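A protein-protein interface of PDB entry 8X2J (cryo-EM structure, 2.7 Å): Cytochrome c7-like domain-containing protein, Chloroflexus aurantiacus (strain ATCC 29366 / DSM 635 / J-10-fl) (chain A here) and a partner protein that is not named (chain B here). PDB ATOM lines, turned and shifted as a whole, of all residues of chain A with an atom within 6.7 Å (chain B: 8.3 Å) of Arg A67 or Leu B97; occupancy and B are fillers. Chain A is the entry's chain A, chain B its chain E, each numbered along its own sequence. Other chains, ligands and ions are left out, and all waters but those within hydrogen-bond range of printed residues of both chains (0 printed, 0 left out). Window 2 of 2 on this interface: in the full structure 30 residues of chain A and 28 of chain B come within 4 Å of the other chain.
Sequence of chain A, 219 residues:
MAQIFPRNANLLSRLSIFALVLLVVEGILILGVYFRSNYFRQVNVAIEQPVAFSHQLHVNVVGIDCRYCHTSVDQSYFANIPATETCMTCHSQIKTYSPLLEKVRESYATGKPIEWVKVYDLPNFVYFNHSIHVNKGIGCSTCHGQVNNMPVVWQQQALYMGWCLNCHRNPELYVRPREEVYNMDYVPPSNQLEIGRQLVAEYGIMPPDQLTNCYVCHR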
ATOM      1  N   ILE A  64      32.698   0.415  26.626  1.00  0.00           N
ATOM      2  CA  ILE A  64      32.221   0.697  25.281  1.00  0.00           C
ATOM      3  C   ILE A  64      30.699   0.718  25.287  1.00  0.00           C
ATOM      4  O   ILE A  64      30.055  -0.179  25.844  1.00  0.00           O
ATOM      5  CB  ILE A  64      32.763  -0.340  24.287  1.00  0.00           C
ATOM      6  CG1 ILE A  64      34.265  -0.539  24.484  1.00  0.00           C
ATOM      7  CG2 ILE A  64      32.518   0.106  22.886  1.00  0.00           C
ATOM      8  CD1 ILE A  64      34.769  -1.862  23.959  1.00  0.00           C
ATOM      9  N   ASP A  65      30.122   1.761  24.693  1.00  0.00           N
ATOM     10  CA  ASP A  65      28.677   1.860  24.561  1.00  0.00           C
ATOM     11  C   ASP A  65      28.159   0.787  23.612  1.00  0.00           C
ATOM     12  O   ASP A  65      28.862   0.344  22.704  1.00  0.00           O
ATOM     13  CB  ASP A  65      28.283   3.246  24.051  1.00  0.00           C
ATOM     14  CG  ASP A  65      26.841   3.593  24.352  1.00  0.00           C
ATOM     15  OD1 ASP A  65      25.942   3.043  23.687  1.00  0.00           O
ATOM     16  OD2 ASP A  65      26.605   4.422  25.254  1.00  0.00           O
ATOM     17  N   CYS A  66      26.911   0.369  23.837  1.00  0.00           N
ATOM     18  CA  CYS A  66      26.327  -0.707  23.044  1.00  0.00           C
ATOM     19  C   CYS A  66      26.093  -0.290  21.596  1.00  0.00           C
ATOM     20  O   CYS A  66      26.142  -1.137  20.698  1.00  0.00           O
ATOM     21  CB  CYS A  66      25.022  -1.182  23.687  1.00  0.00           C
ATOM     22  SG  CYS A  66      25.152  -1.608  25.452  1.00  0.00           S
ATOM     23  N   ARG A  67      25.856   1.000  21.345  1.00  0.00           N
ATOM     24  CA  ARG A  67      25.677   1.497  19.985  1.00  0.00           C
ATOM     25  C   ARG A  67      26.985   1.685  19.233  1.00  0.00           C
ATOM     26  O   ARG A  67      26.945   1.945  18.026  1.00  0.00           O
ATOM     27  CB  ARG A  67      24.934   2.832  19.987  1.00  0.00           C
ATOM     28  CG  ARG A  67      23.437   2.740  20.059  1.00  0.00           C
ATOM     29  CD  ARG A  67      22.880   4.033  20.616  1.00  0.00           C
ATOM     30  NE  ARG A  67      23.296   4.241  21.998  1.00  0.00           N
ATOM     31  CZ  ARG A  67      22.938   5.279  22.738  1.00  0.00           C
ATOM     32  NH1 ARG A  67      22.126   6.212  22.272  1.00  0.00           N
ATOM     33  NH2 ARG A  67      23.405   5.383  23.979  1.00  0.00           N
ATOM     34  N   TYR A  68      28.131   1.611  19.915  1.00  0.00           N
ATOM     35  CA  TYR A  68      29.414   1.654  19.222  1.00  0.00           C
ATOM     36  C   TYR A  68      29.585   0.436  18.330  1.00  0.00           C
ATOM     37  O   TYR A  68      30.139   0.534  17.229  1.00  0.00           O
ATOM     38  CB  TYR A  68      30.553   1.741  20.238  1.00  0.00           C
ATOM     39  CG  TYR A  68      31.952   1.869  19.661  1.00  0.00           C
ATOM     40  CD1 TYR A  68      32.729   0.745  19.386  1.00  0.00           C
ATOM     41  CD2 TYR A  68      32.512   3.116  19.431  1.00  0.00           C
ATOM     42  CE1 TYR A  68      34.002   0.863  18.876  1.00  0.00           C
ATOM     43  CE2 TYR A  68      33.788   3.243  18.923  1.00  0.00           C
ATOM     44  CZ  TYR A  68      34.526   2.113  18.648  1.00  0.00           C
ATOM     45  OH  TYR A  68      35.798   2.229  18.142  1.00  0.00           O
ATOM     46  N   CYS A  69      29.121  -0.716  18.796  1.00  0.00           N
ATOM     47  CA  CYS A  69      29.268  -1.974  18.084  1.00  0.00           C
ATOM     48  C   CYS A  69      27.971  -2.448  17.447  1.00  0.00           C
ATOM     49  O   CYS A  69      27.989  -2.940  16.316  1.00  0.00           O
ATOM     50  CB  CYS A  69      29.810  -3.029  19.042  1.00  0.00           C
ATOM     51  SG  CYS A  69      31.558  -2.797  19.414  1.00  0.00           S
ATOM     52  N   HIS A  70      26.839  -2.302  18.134  1.00  0.00           N
ATOM     53  CA  HIS A  70      25.530  -2.578  17.548  1.00  0.00           C
ATOM     54  C   HIS A  70      24.947  -1.243  17.096  1.00  0.00           C
ATOM     55  O   HIS A  70      24.063  -0.667  17.726  1.00  0.00           O
ATOM     56  CB  HIS A  70      24.640  -3.302  18.547  1.00  0.00           C
ATOM     57  CG  HIS A  70      25.343  -4.397  19.285  1.00  0.00           C
ATOM     58  ND1 HIS A  70      25.745  -5.565  18.675  1.00  0.00           N
ATOM     59  CD2 HIS A  70      25.740  -4.491  20.575  1.00  0.00           C
ATOM     60  CE1 HIS A  70      26.345  -6.338  19.561  1.00  0.00           C
ATOM     61  NE2 HIS A  70      26.356  -5.708  20.722  1.00  0.00           N
ATOM     62  N   THR A  71      25.473  -0.753  15.972  1.00  0.00           N
ATOM     63  CA  THR A  71      25.192   0.602  15.521  1.00  0.00           C
ATOM     64  C   THR A  71      23.796   0.758  14.937  1.00  0.00           C
ATOM     65  O   THR A  71      23.271   1.875  14.911  1.00  0.00           O
ATOM     66  CB  THR A  71      26.231   1.026  14.483  1.00  0.00           C
ATOM     67  OG1 THR A  71      25.998   0.321  13.259  1.00  0.00           O
ATOM     68  CG2 THR A  71      27.627   0.708  14.972  1.00  0.00           C
ATOM     69  N   SER A  72      23.181  -0.329  14.476  1.00  0.00           N
ATOM     70  CA  SER A  72      21.920  -0.264  13.755  1.00  0.00           C
ATOM     71  C   SER A  72      20.728  -0.662  14.616  1.00  0.00           C
ATOM     72  O   SER A  72      19.662  -0.974  14.077  1.00  0.00           O
ATOM     73  CB  SER A  72      21.991  -1.149  12.513  1.00  0.00           C
ATOM     74  OG  SER A  72      20.699  -1.484  12.049  1.00  0.00           O
ATOM     75  N   VAL A  73      20.881  -0.649  15.939  1.00  0.00           N
ATOM     76  CA  VAL A  73      19.842  -1.209  16.795  1.00  0.00           C
ATOM     77  C   VAL A  73      18.689  -0.224  16.992  1.00  0.00           C
ATOM     78  O   VAL A  73      17.543  -0.639  17.203  1.00  0.00           O
ATOM     79  CB  VAL A  73      20.466  -1.678  18.126  1.00  0.00           C
ATOM     80  CG1 VAL A  73      20.943  -0.509  18.979  1.00  0.00           C
ATOM     81  CG2 VAL A  73      19.515  -2.577  18.889  1.00  0.00           C
ATOM     82  N   ASP A  74      18.941   1.078  16.881  1.00  0.00           N
ATOM     83  CA  ASP A  74      17.907   2.087  17.048  1.00  0.00           C
ATOM     84  C   ASP A  74      17.389   2.620  15.722  1.00  0.00           C
ATOM     85  O   ASP A  74      16.645   3.605  15.711  1.00  0.00           O
ATOM     86  CB  ASP A  74      18.430   3.240  17.905  1.00  0.00           C
ATOM     87  CG  ASP A  74      19.609   3.950  17.270  1.00  0.00           C
ATOM     88  OD1 ASP A  74      20.480   3.266  16.693  1.00  0.00           O
ATOM     89  OD2 ASP A  74      19.671   5.195  17.353  1.00  0.00           O
ATOM     90  N   TYR A 182      19.667   2.153  27.170  1.00  0.00           N
ATOM     91  CA  TYR A 182      21.056   1.750  27.049  1.00  0.00           C
ATOM     92  C   TYR A 182      21.770   1.702  28.389  1.00  0.00           C
ATOM     93  O   TYR A 182      22.935   1.293  28.440  1.00  0.00           O
ATOM     94  CB  TYR A 182      21.776   2.707  26.105  1.00  0.00           C
ATOM     95  CG  TYR A 182      21.203   2.661  24.717  1.00  0.00           C
ATOM     96  CD1 TYR A 182      21.607   1.690  23.818  1.00  0.00           C
ATOM     97  CD2 TYR A 182      20.242   3.580  24.308  1.00  0.00           C
ATOM     98  CE1 TYR A 182      21.084   1.641  22.555  1.00  0.00           C
ATOM     99  CE2 TYR A 182      19.709   3.534  23.041  1.00  0.00           C
ATOM    100  CZ  TYR A 182      20.133   2.557  22.171  1.00  0.00           C
ATOM    101  OH  TYR A 182      19.628   2.500  20.899  1.00  0.00           O
ATOM    102  N   ASP B  90      19.578  21.302  19.068  1.00  0.00           N
ATOM    103  CA  ASP B  90      19.284  19.895  18.805  1.00  0.00           C
ATOM    104  C   ASP B  90      20.448  19.206  18.103  1.00  0.00           C
ATOM    105  O   ASP B  90      20.748  18.038  18.386  1.00  0.00           O
ATOM    106  CB  ASP B  90      18.006  19.772  17.975  1.00  0.00           C
ATOM    107  CG  ASP B  90      16.773  20.222  18.733  1.00  0.00           C
ATOM    108  OD1 ASP B  90      16.780  20.150  19.980  1.00  0.00           O
ATOM    109  OD2 ASP B  90      15.797  20.648  18.082  1.00  0.00           O
ATOM    110  N   LEU B  91      21.119  19.922  17.194  1.00  0.00           N
ATOM    111  CA  LEU B  91      22.311  19.388  16.538  1.00  0.00           C
ATOM    112  C   LEU B  91      23.443  19.172  17.534  1.00  0.00           C
ATOM    113  O   LEU B  91      24.166  18.174  17.456  1.00  0.00           O
ATOM    114  CB  LEU B  91      22.754  20.333  15.421  1.00  0.00           C
ATOM    115  CG  LEU B  91      24.018  19.963  14.646  1.00  0.00           C
ATOM    116  CD1 LEU B  91      23.691  19.000  13.516  1.00  0.00           C
ATOM    117  CD2 LEU B  91      24.696  21.211  14.115  1.00  0.00           C
ATOM    118  N   LEU B  92      23.601  20.092  18.487  1.00  0.00           N
ATOM    119  CA  LEU B  92      24.624  19.942  19.517  1.00  0.00           C
ATOM    120  C   LEU B  92      24.302  18.802  20.474  1.00  0.00           C
ATOM    121  O   LEU B  92      25.215  18.117  20.942  1.00  0.00           O
ATOM    122  CB  LEU B  92      24.785  21.252  20.285  1.00  0.00           C
ATOM    123  CG  LEU B  92      25.904  22.177  19.813  1.00  0.00           C
ATOM    124  CD1 LEU B  92      25.834  23.496  20.546  1.00  0.00           C
ATOM    125  CD2 LEU B  92      27.251  21.523  20.031  1.00  0.00           C
ATOM    126  N   LEU B  93      23.019  18.578  20.769  1.00  0.00           N
ATOM    127  CA  LEU B  93      22.639  17.437  21.598  1.00  0.00           C
ATOM    128  C   LEU B  93      22.869  16.116  20.867  1.00  0.00           C
ATOM    129  O   LEU B  93      23.307  15.130  21.476  1.00  0.00           O
ATOM    130  CB  LEU B  93      21.181  17.569  22.035  1.00  0.00           C
ATOM    131  CG  LEU B  93      20.912  18.580  23.151  1.00  0.00           C
ATOM    132  CD1 LEU B  93      19.424  18.846  23.286  1.00  0.00           C
ATOM    133  CD2 LEU B  93      21.489  18.091  24.466  1.00  0.00           C
ATOM    134  N   ARG B  94      22.590  16.084  19.559  1.00  0.00           N
ATOM    135  CA  ARG B  94      22.897  14.906  18.749  1.00  0.00           C
ATOM    136  C   ARG B  94      24.401  14.662  18.676  1.00  0.00           C
ATOM    137  O   ARG B  94      24.857  13.512  18.721  1.00  0.00           O
ATOM    138  CB  ARG B  94      22.304  15.073  17.347  1.00  0.00           C
ATOM    139  CG  ARG B  94      22.625  13.947  16.377  1.00  0.00           C
ATOM    140  CD  ARG B  94      21.916  12.659  16.760  1.00  0.00           C
ATOM    141  NE  ARG B  94      20.479  12.740  16.526  1.00  0.00           N
ATOM    142  CZ  ARG B  94      19.598  11.843  16.946  1.00  0.00           C
ATOM    143  NH1 ARG B  94      19.973  10.774  17.628  1.00  0.00           N
ATOM    144  NH2 ARG B  94      18.308  12.025  16.676  1.00  0.00           N
ATOM    145  N   GLY B  95      25.186  15.737  18.578  1.00  0.00           N
ATOM    146  CA  GLY B  95      26.632  15.601  18.599  1.00  0.00           C
ATOM    147  C   GLY B  95      27.165  15.125  19.934  1.00  0.00           C
ATOM    148  O   GLY B  95      28.126  14.357  19.982  1.00  0.00           O
ATOM    149  N   GLN B  96      26.548  15.569  21.033  1.00  0.00           N
ATOM    150  CA  GLN B  96      26.906  15.068  22.356  1.00  0.00           C
ATOM    151  C   GLN B  96      26.595  13.583  22.488  1.00  0.00           C
ATOM    152  O   GLN B  96      27.401  12.817  23.032  1.00  0.00           O
ATOM    153  CB  GLN B  96      26.170  15.864  23.434  1.00  0.00           C
ATOM    154  CG  GLN B  96      26.411  15.371  24.852  1.00  0.00           C
ATOM    155  CD  GLN B  96      25.544  16.072  25.872  1.00  0.00           C
ATOM    156  OE1 GLN B  96      24.564  16.729  25.527  1.00  0.00           O
ATOM    157  NE2 GLN B  96      25.903  15.938  27.143  1.00  0.00           N
ATOM    158  N   LEU B  97      25.436  13.158  21.969  1.00  0.00           N
ATOM    159  CA  LEU B  97      25.064  11.745  22.006  1.00  0.00           C
ATOM    160  C   LEU B  97      26.018  10.888  21.179  1.00  0.00           C
ATOM    161  O   LEU B  97      26.479   9.838  21.641  1.00  0.00           O
ATOM    162  CB  LEU B  97      23.632  11.572  21.504  1.00  0.00           C
ATOM    163  CG  LEU B  97      23.127  10.133  21.415  1.00  0.00           C
ATOM    164  CD1 LEU B  97      22.919   9.556  22.803  1.00  0.00           C
ATOM    165  CD2 LEU B  97      21.849  10.061  20.598  1.00  0.00           C
ATOM    166  N   LYS B  98      26.349  11.338  19.966  1.00  0.00           N
ATOM    167  CA  LYS B  98      27.247  10.569  19.113  1.00  0.00           C
ATOM    168  C   LYS B  98      28.684  10.598  19.625  1.00  0.00           C
ATOM    169  O   LYS B  98      29.429   9.634  19.417  1.00  0.00           O
ATOM    170  CB  LYS B  98      27.175  11.091  17.680  1.00  0.00           C
ATOM    171  CG  LYS B  98      25.929  10.671  16.928  1.00  0.00           C
ATOM    172  CD  LYS B  98      25.864   9.168  16.773  1.00  0.00           C
ATOM    173  CE  LYS B  98      24.505   8.723  16.274  1.00  0.00           C
ATOM    174  NZ  LYS B  98      23.569   8.452  17.393  1.00  0.00           N
ATOM    175  N   TYR B  99      29.084  11.683  20.295  1.00  0.00           N
ATOM    176  CA  TYR B  99      30.378  11.722  20.967  1.00  0.00           C
ATOM    177  C   TYR B  99      30.430  10.723  22.114  1.00  0.00           C
ATOM    178  O   TYR B  99      31.448  10.051  22.313  1.00  0.00           O
ATOM    179  CB  TYR B  99      30.654  13.140  21.475  1.00  0.00           C
ATOM    180  CG  TYR B  99      31.945  13.296  22.252  1.00  0.00           C
ATOM    181  CD1 TYR B  99      33.143  13.521  21.595  1.00  0.00           C
ATOM    182  CD2 TYR B  99      31.960  13.247  23.644  1.00  0.00           C
ATOM    183  CE1 TYR B  99      34.323  13.655  22.291  1.00  0.00           C
ATOM    184  CE2 TYR B  99      33.134  13.385  24.347  1.00  0.00           C
ATOM    185  CZ  TYR B  99      34.311  13.593  23.665  1.00  0.00           C
ATOM    186  OH  TYR B  99      35.482  13.734  24.361  1.00  0.00           O
ATOM    187  N   ASN B 100      29.351  10.635  22.899  1.00  0.00           N
ATOM    188  CA  ASN B 100      29.322   9.688  24.007  1.00  0.00           C
ATOM    189  C   ASN B 100      29.265   8.248  23.515  1.00  0.00           C
ATOM    190  O   ASN B 100      29.762   7.343  24.194  1.00  0.00           O
ATOM    191  CB  ASN B 100      28.136   9.986  24.922  1.00  0.00           C
ATOM    192  CG  ASN B 100      28.287  11.300  25.661  1.00  0.00           C
ATOM    193  OD1 ASN B 100      29.236  12.047  25.434  1.00  0.00           O
ATOM    194  ND2 ASN B 100      27.343  11.591  26.548  1.00  0.00           N
ATOM    195  N   ILE B 101      28.671   8.018  22.347  1.00  0.00           N
ATOM    196  CA  ILE B 101      28.629   6.670  21.788  1.00  0.00           C
ATOM    197  C   ILE B 101      29.987   6.277  21.216  1.00  0.00           C
ATOM    198  O   ILE B 101      30.565   5.253  21.597  1.00  0.00           O
ATOM    199  CB  ILE B 101      27.524   6.561  20.721  1.00  0.00           C
ATOM    200  CG1 ILE B 101      26.144   6.577  21.368  1.00  0.00           C
ATOM    201  CG2 ILE B 101      27.683   5.289  19.917  1.00  0.00           C
ATOM    202  CD1 ILE B 101      25.062   7.040  20.432  1.00  0.00           C
ATOM    203  N   TYR B 102      30.523   7.090  20.305  1.00  0.00           N
ATOM    204  CA  TYR B 102      31.632   6.662  19.462  1.00  0.00           C
ATOM    205  C   TYR B 102      32.984   7.225  19.867  1.00  0.00           C
ATOM    206  O   TYR B 102      34.007   6.605  19.565  1.00  0.00           O
ATOM    207  CB  TYR B 102      31.365   7.044  18.004  1.00  0.00           C
ATOM    208  CG  TYR B 102      30.216   6.292  17.380  1.00  0.00           C
ATOM    209  CD1 TYR B 102      30.279   4.917  17.203  1.00  0.00           C
ATOM    210  CD2 TYR B 102      29.066   6.955  16.973  1.00  0.00           C
ATOM    211  CE1 TYR B 102      29.231   4.224  16.635  1.00  0.00           C
ATOM    212  CE2 TYR B 102      28.012   6.269  16.406  1.00  0.00           C
ATOM    213  CZ  TYR B 102      28.100   4.903  16.241  1.00  0.00           C
ATOM    214  OH  TYR B 102      27.053   4.215  15.675  1.00  0.00           O
ATOM    215  N   CYS B 103      33.029   8.374  20.534  1.00  0.00           N
ATOM    216  CA  CYS B 103      34.292   9.073  20.726  1.00  0.00           C
ATOM    217  C   CYS B 103      34.745   9.153  22.172  1.00  0.00           C
ATOM    218  O   CYS B 103      35.945   9.277  22.420  1.00  0.00           O
ATOM    219  CB  CYS B 103      34.194  10.494  20.169  1.00  0.00           C
ATOM    220  SG  CYS B 103      33.331  10.630  18.598  1.00  0.00           S
ATOM    221  N   ALA B 104      33.826   9.079  23.132  1.00  0.00           N
ATOM    222  CA  ALA B 104      34.170   9.226  24.539  1.00  0.00           C
ATOM    223  C   ALA B 104      34.745   7.956  25.150  1.00  0.00           C
ATOM    224  O   ALA B 104      35.117   7.972  26.328  1.00  0.00           O
ATOM    225  CB  ALA B 104      32.942   9.670  25.336  1.00  0.00           C
ATOM    226  N   GLU B 109      34.760  11.527  28.287  1.00  0.00           N
ATOM    227  CA  GLU B 109      33.550  12.338  28.188  1.00  0.00           C
ATOM    228  C   GLU B 109      33.880  13.826  28.186  1.00  0.00           C
ATOM    229  O   GLU B 109      33.282  14.598  27.429  1.00  0.00           O
ATOM    230  CB  GLU B 109      32.596  12.004  29.334  1.00  0.00           C
ATOM    231  CG  GLU B 109      32.111  10.565  29.356  1.00  0.00           C
ATOM    232  CD  GLU B 109      30.755  10.399  28.704  1.00  0.00           C
ATOM    233  OE1 GLU B 109      30.144  11.422  28.334  1.00  0.00           O
ATOM    234  OE2 GLU B 109      30.295   9.246  28.570  1.00  0.00           O
ATOM    235  N   ARG B 168      30.805   4.206  10.210  1.00  0.00           N
ATOM    236  CA  ARG B 168      29.838   4.074  11.291  1.00  0.00           C
ATOM    237  C   ARG B 168      28.984   5.315  11.500  1.00  0.00           C
ATOM    238  O   ARG B 168      27.849   5.198  11.977  1.00  0.00           O
ATOM    239  CB  ARG B 168      30.554   3.733  12.603  1.00  0.00           C
ATOM    240  CG  ARG B 168      30.891   2.261  12.753  1.00  0.00           C
ATOM    241  CD  ARG B 168      31.622   1.974  14.059  1.00  0.00           C
ATOM    242  NE  ARG B 168      32.991   2.477  14.067  1.00  0.00           N
ATOM    243  CZ  ARG B 168      34.021   1.865  13.498  1.00  0.00           C
ATOM    244  NH1 ARG B 168      33.875   0.724  12.844  1.00  0.00           N
ATOM    245  NH2 ARG B 168      35.230   2.411  13.586  1.00  0.00           N
ATOM    246  N   ILE B 169      29.490   6.499  11.161  1.00  0.00           N
ATOM    247  CA  ILE B 169      28.831   7.757  11.488  1.00  0.00           C
ATOM    248  C   ILE B 169      28.445   8.474  10.200  1.00  0.00           C
ATOM    249  O   ILE B 169      29.265   8.605   9.283  1.00  0.00           O
ATOM    250  CB  ILE B 169      29.722   8.653  12.369  1.00  0.00           C
ATOM    251  CG1 ILE B 169      30.424   7.829  13.449  1.00  0.00           C
ATOM    252  CG2 ILE B 169      28.893   9.718  13.036  1.00  0.00           C
ATOM    253  CD1 ILE B 169      31.332   8.636  14.344  1.00  0.00           C
ATOM    254  N   ASP B 173      26.159  13.755  11.298  1.00  0.00           N
ATOM    255  CA  ASP B 173      26.469  13.466  12.693  1.00  0.00           C
ATOM    256  C   ASP B 173      27.946  13.681  13.001  1.00  0.00           C
ATOM    257  O   ASP B 173      28.287  14.015  14.137  1.00  0.00           O
ATOM    258  CB  ASP B 173      26.046  12.041  13.039  1.00  0.00           C
ATOM    259  CG  ASP B 173      24.611  11.748  12.655  1.00  0.00           C
ATOM    260  OD1 ASP B 173      23.853  12.709  12.409  1.00  0.00           O
ATOM    261  OD2 ASP B 173      24.241  10.557  12.597  1.00  0.00           O
ATOM    262  N   ALA B 176      28.123  17.281  13.590  1.00  0.00           N
ATOM    263  CA  ALA B 176      27.570  17.510  14.924  1.00  0.00           C
ATOM    264  C   ALA B 176      28.571  17.144  16.018  1.00  0.00           C
ATOM    265  O   ALA B 176      28.641  17.818  17.054  1.00  0.00           O
ATOM    266  CB  ALA B 176      26.275  16.717  15.088  1.00  0.00           C
ATOM    267  N   ILE B 177      29.349  16.078  15.802  1.00  0.00           N
ATOM    268  CA  ILE B 177      30.410  15.697  16.730  1.00  0.00           C
ATOM    269  C   ILE B 177      31.480  16.782  16.791  1.00  0.00           C
ATOM    270  O   ILE B 177      31.967  17.131  17.871  1.00  0.00           O
ATOM    271  CB  ILE B 177      30.998  14.326  16.331  1.00  0.00           C
ATOM    272  CG1 ILE B 177      30.066  13.194  16.745  1.00  0.00           C
ATOM    273  CG2 ILE B 177      32.333  14.066  16.992  1.00  0.00           C
ATOM    274  CD1 ILE B 177      30.494  11.846  16.216  1.00  0.00           C
ATOM    275  N   TYR B 180      30.163  19.577  18.833  1.00  0.00           N
ATOM    276  CA  TYR B 180      30.278  19.262  20.255  1.00  0.00           C
ATOM    277  C   TYR B 180      31.726  19.305  20.735  1.00  0.00           C
ATOM    278  O   TYR B 180      31.974  19.573  21.915  1.00  0.00           O
ATOM    279  CB  TYR B 180      29.663  17.897  20.558  1.00  0.00           C
ATOM    280  CG  TYR B 180      29.583  17.620  22.041  1.00  0.00           C
ATOM    281  CD1 TYR B 180      28.848  18.446  22.883  1.00  0.00           C
ATOM    282  CD2 TYR B 180      30.278  16.559  22.604  1.00  0.00           C
ATOM    283  CE1 TYR B 180      28.789  18.207  24.242  1.00  0.00           C
ATOM    284  CE2 TYR B 180      30.220  16.309  23.960  1.00  0.00           C
ATOM    285  CZ  TYR B 180      29.478  17.136  24.773  1.00  0.00           C
ATOM    286  OH  TYR B 180      29.424  16.885  26.124  1.00  0.00           O
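O of Arg A67 is in hydrogen-bond range of OH of Tyr B102, 3.3 Å away.
Of chain B, only Leu B97, Ile B101 and Tyr B102 come within 4 Å of Arg A67.
Printed residues of chain B within 4 Å of Thr A71: Tyr B102 (3.5 Å).
Leu B97 touches one residue of chain A.
Printed residues of chain A within 4 Å of Ile B101: Asp A65, Arg A67 and Tyr A68.
Of the printed residues of chain A, Tyr B102 touches Arg A67 (3.3 Å), Tyr A68 (3.4 Å) and Thr A71 (3.5 Å).
Printed residues of chain A within 4 Å of Arg B168: Tyr A68.
The nearest residue of chain A that does not touch Leu B97 is Asp A74 (6.2 Å).
The nearest printed residue of chain A that does not touch Arg B168 is Thr A71 (4.2 Å).
Hydrophobic or aromatic side chains of chain B that line the printed part of chain A: Leu B97, Ile B101 and Tyr B102.
Along chain A the printed residues that touch a printed residue of chain B span positions 65 to 71.
Among the printed residues, 8 pairs touch across the chains.
Asp A65 touches Ile B101.
Arg A67 touches Leu B97 (NH1 to CD1, 3.5 Å).
CD1 of Ile B101 touches NH1 of Arg A67, at 3.6 Å.
Ile B101 touches Tyr A68.
Tyr A68 touches Tyr B102.
Tyr A68 touches Arg B168.
CB of Thr A71 touches OH of Tyr B102, 3.5 Å away.
The side-chain carboxylate (OD1) of Asp A65 lies within salt-bridge range of the guanidinium group (NE) of Arg A67, at 3.4 Å.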
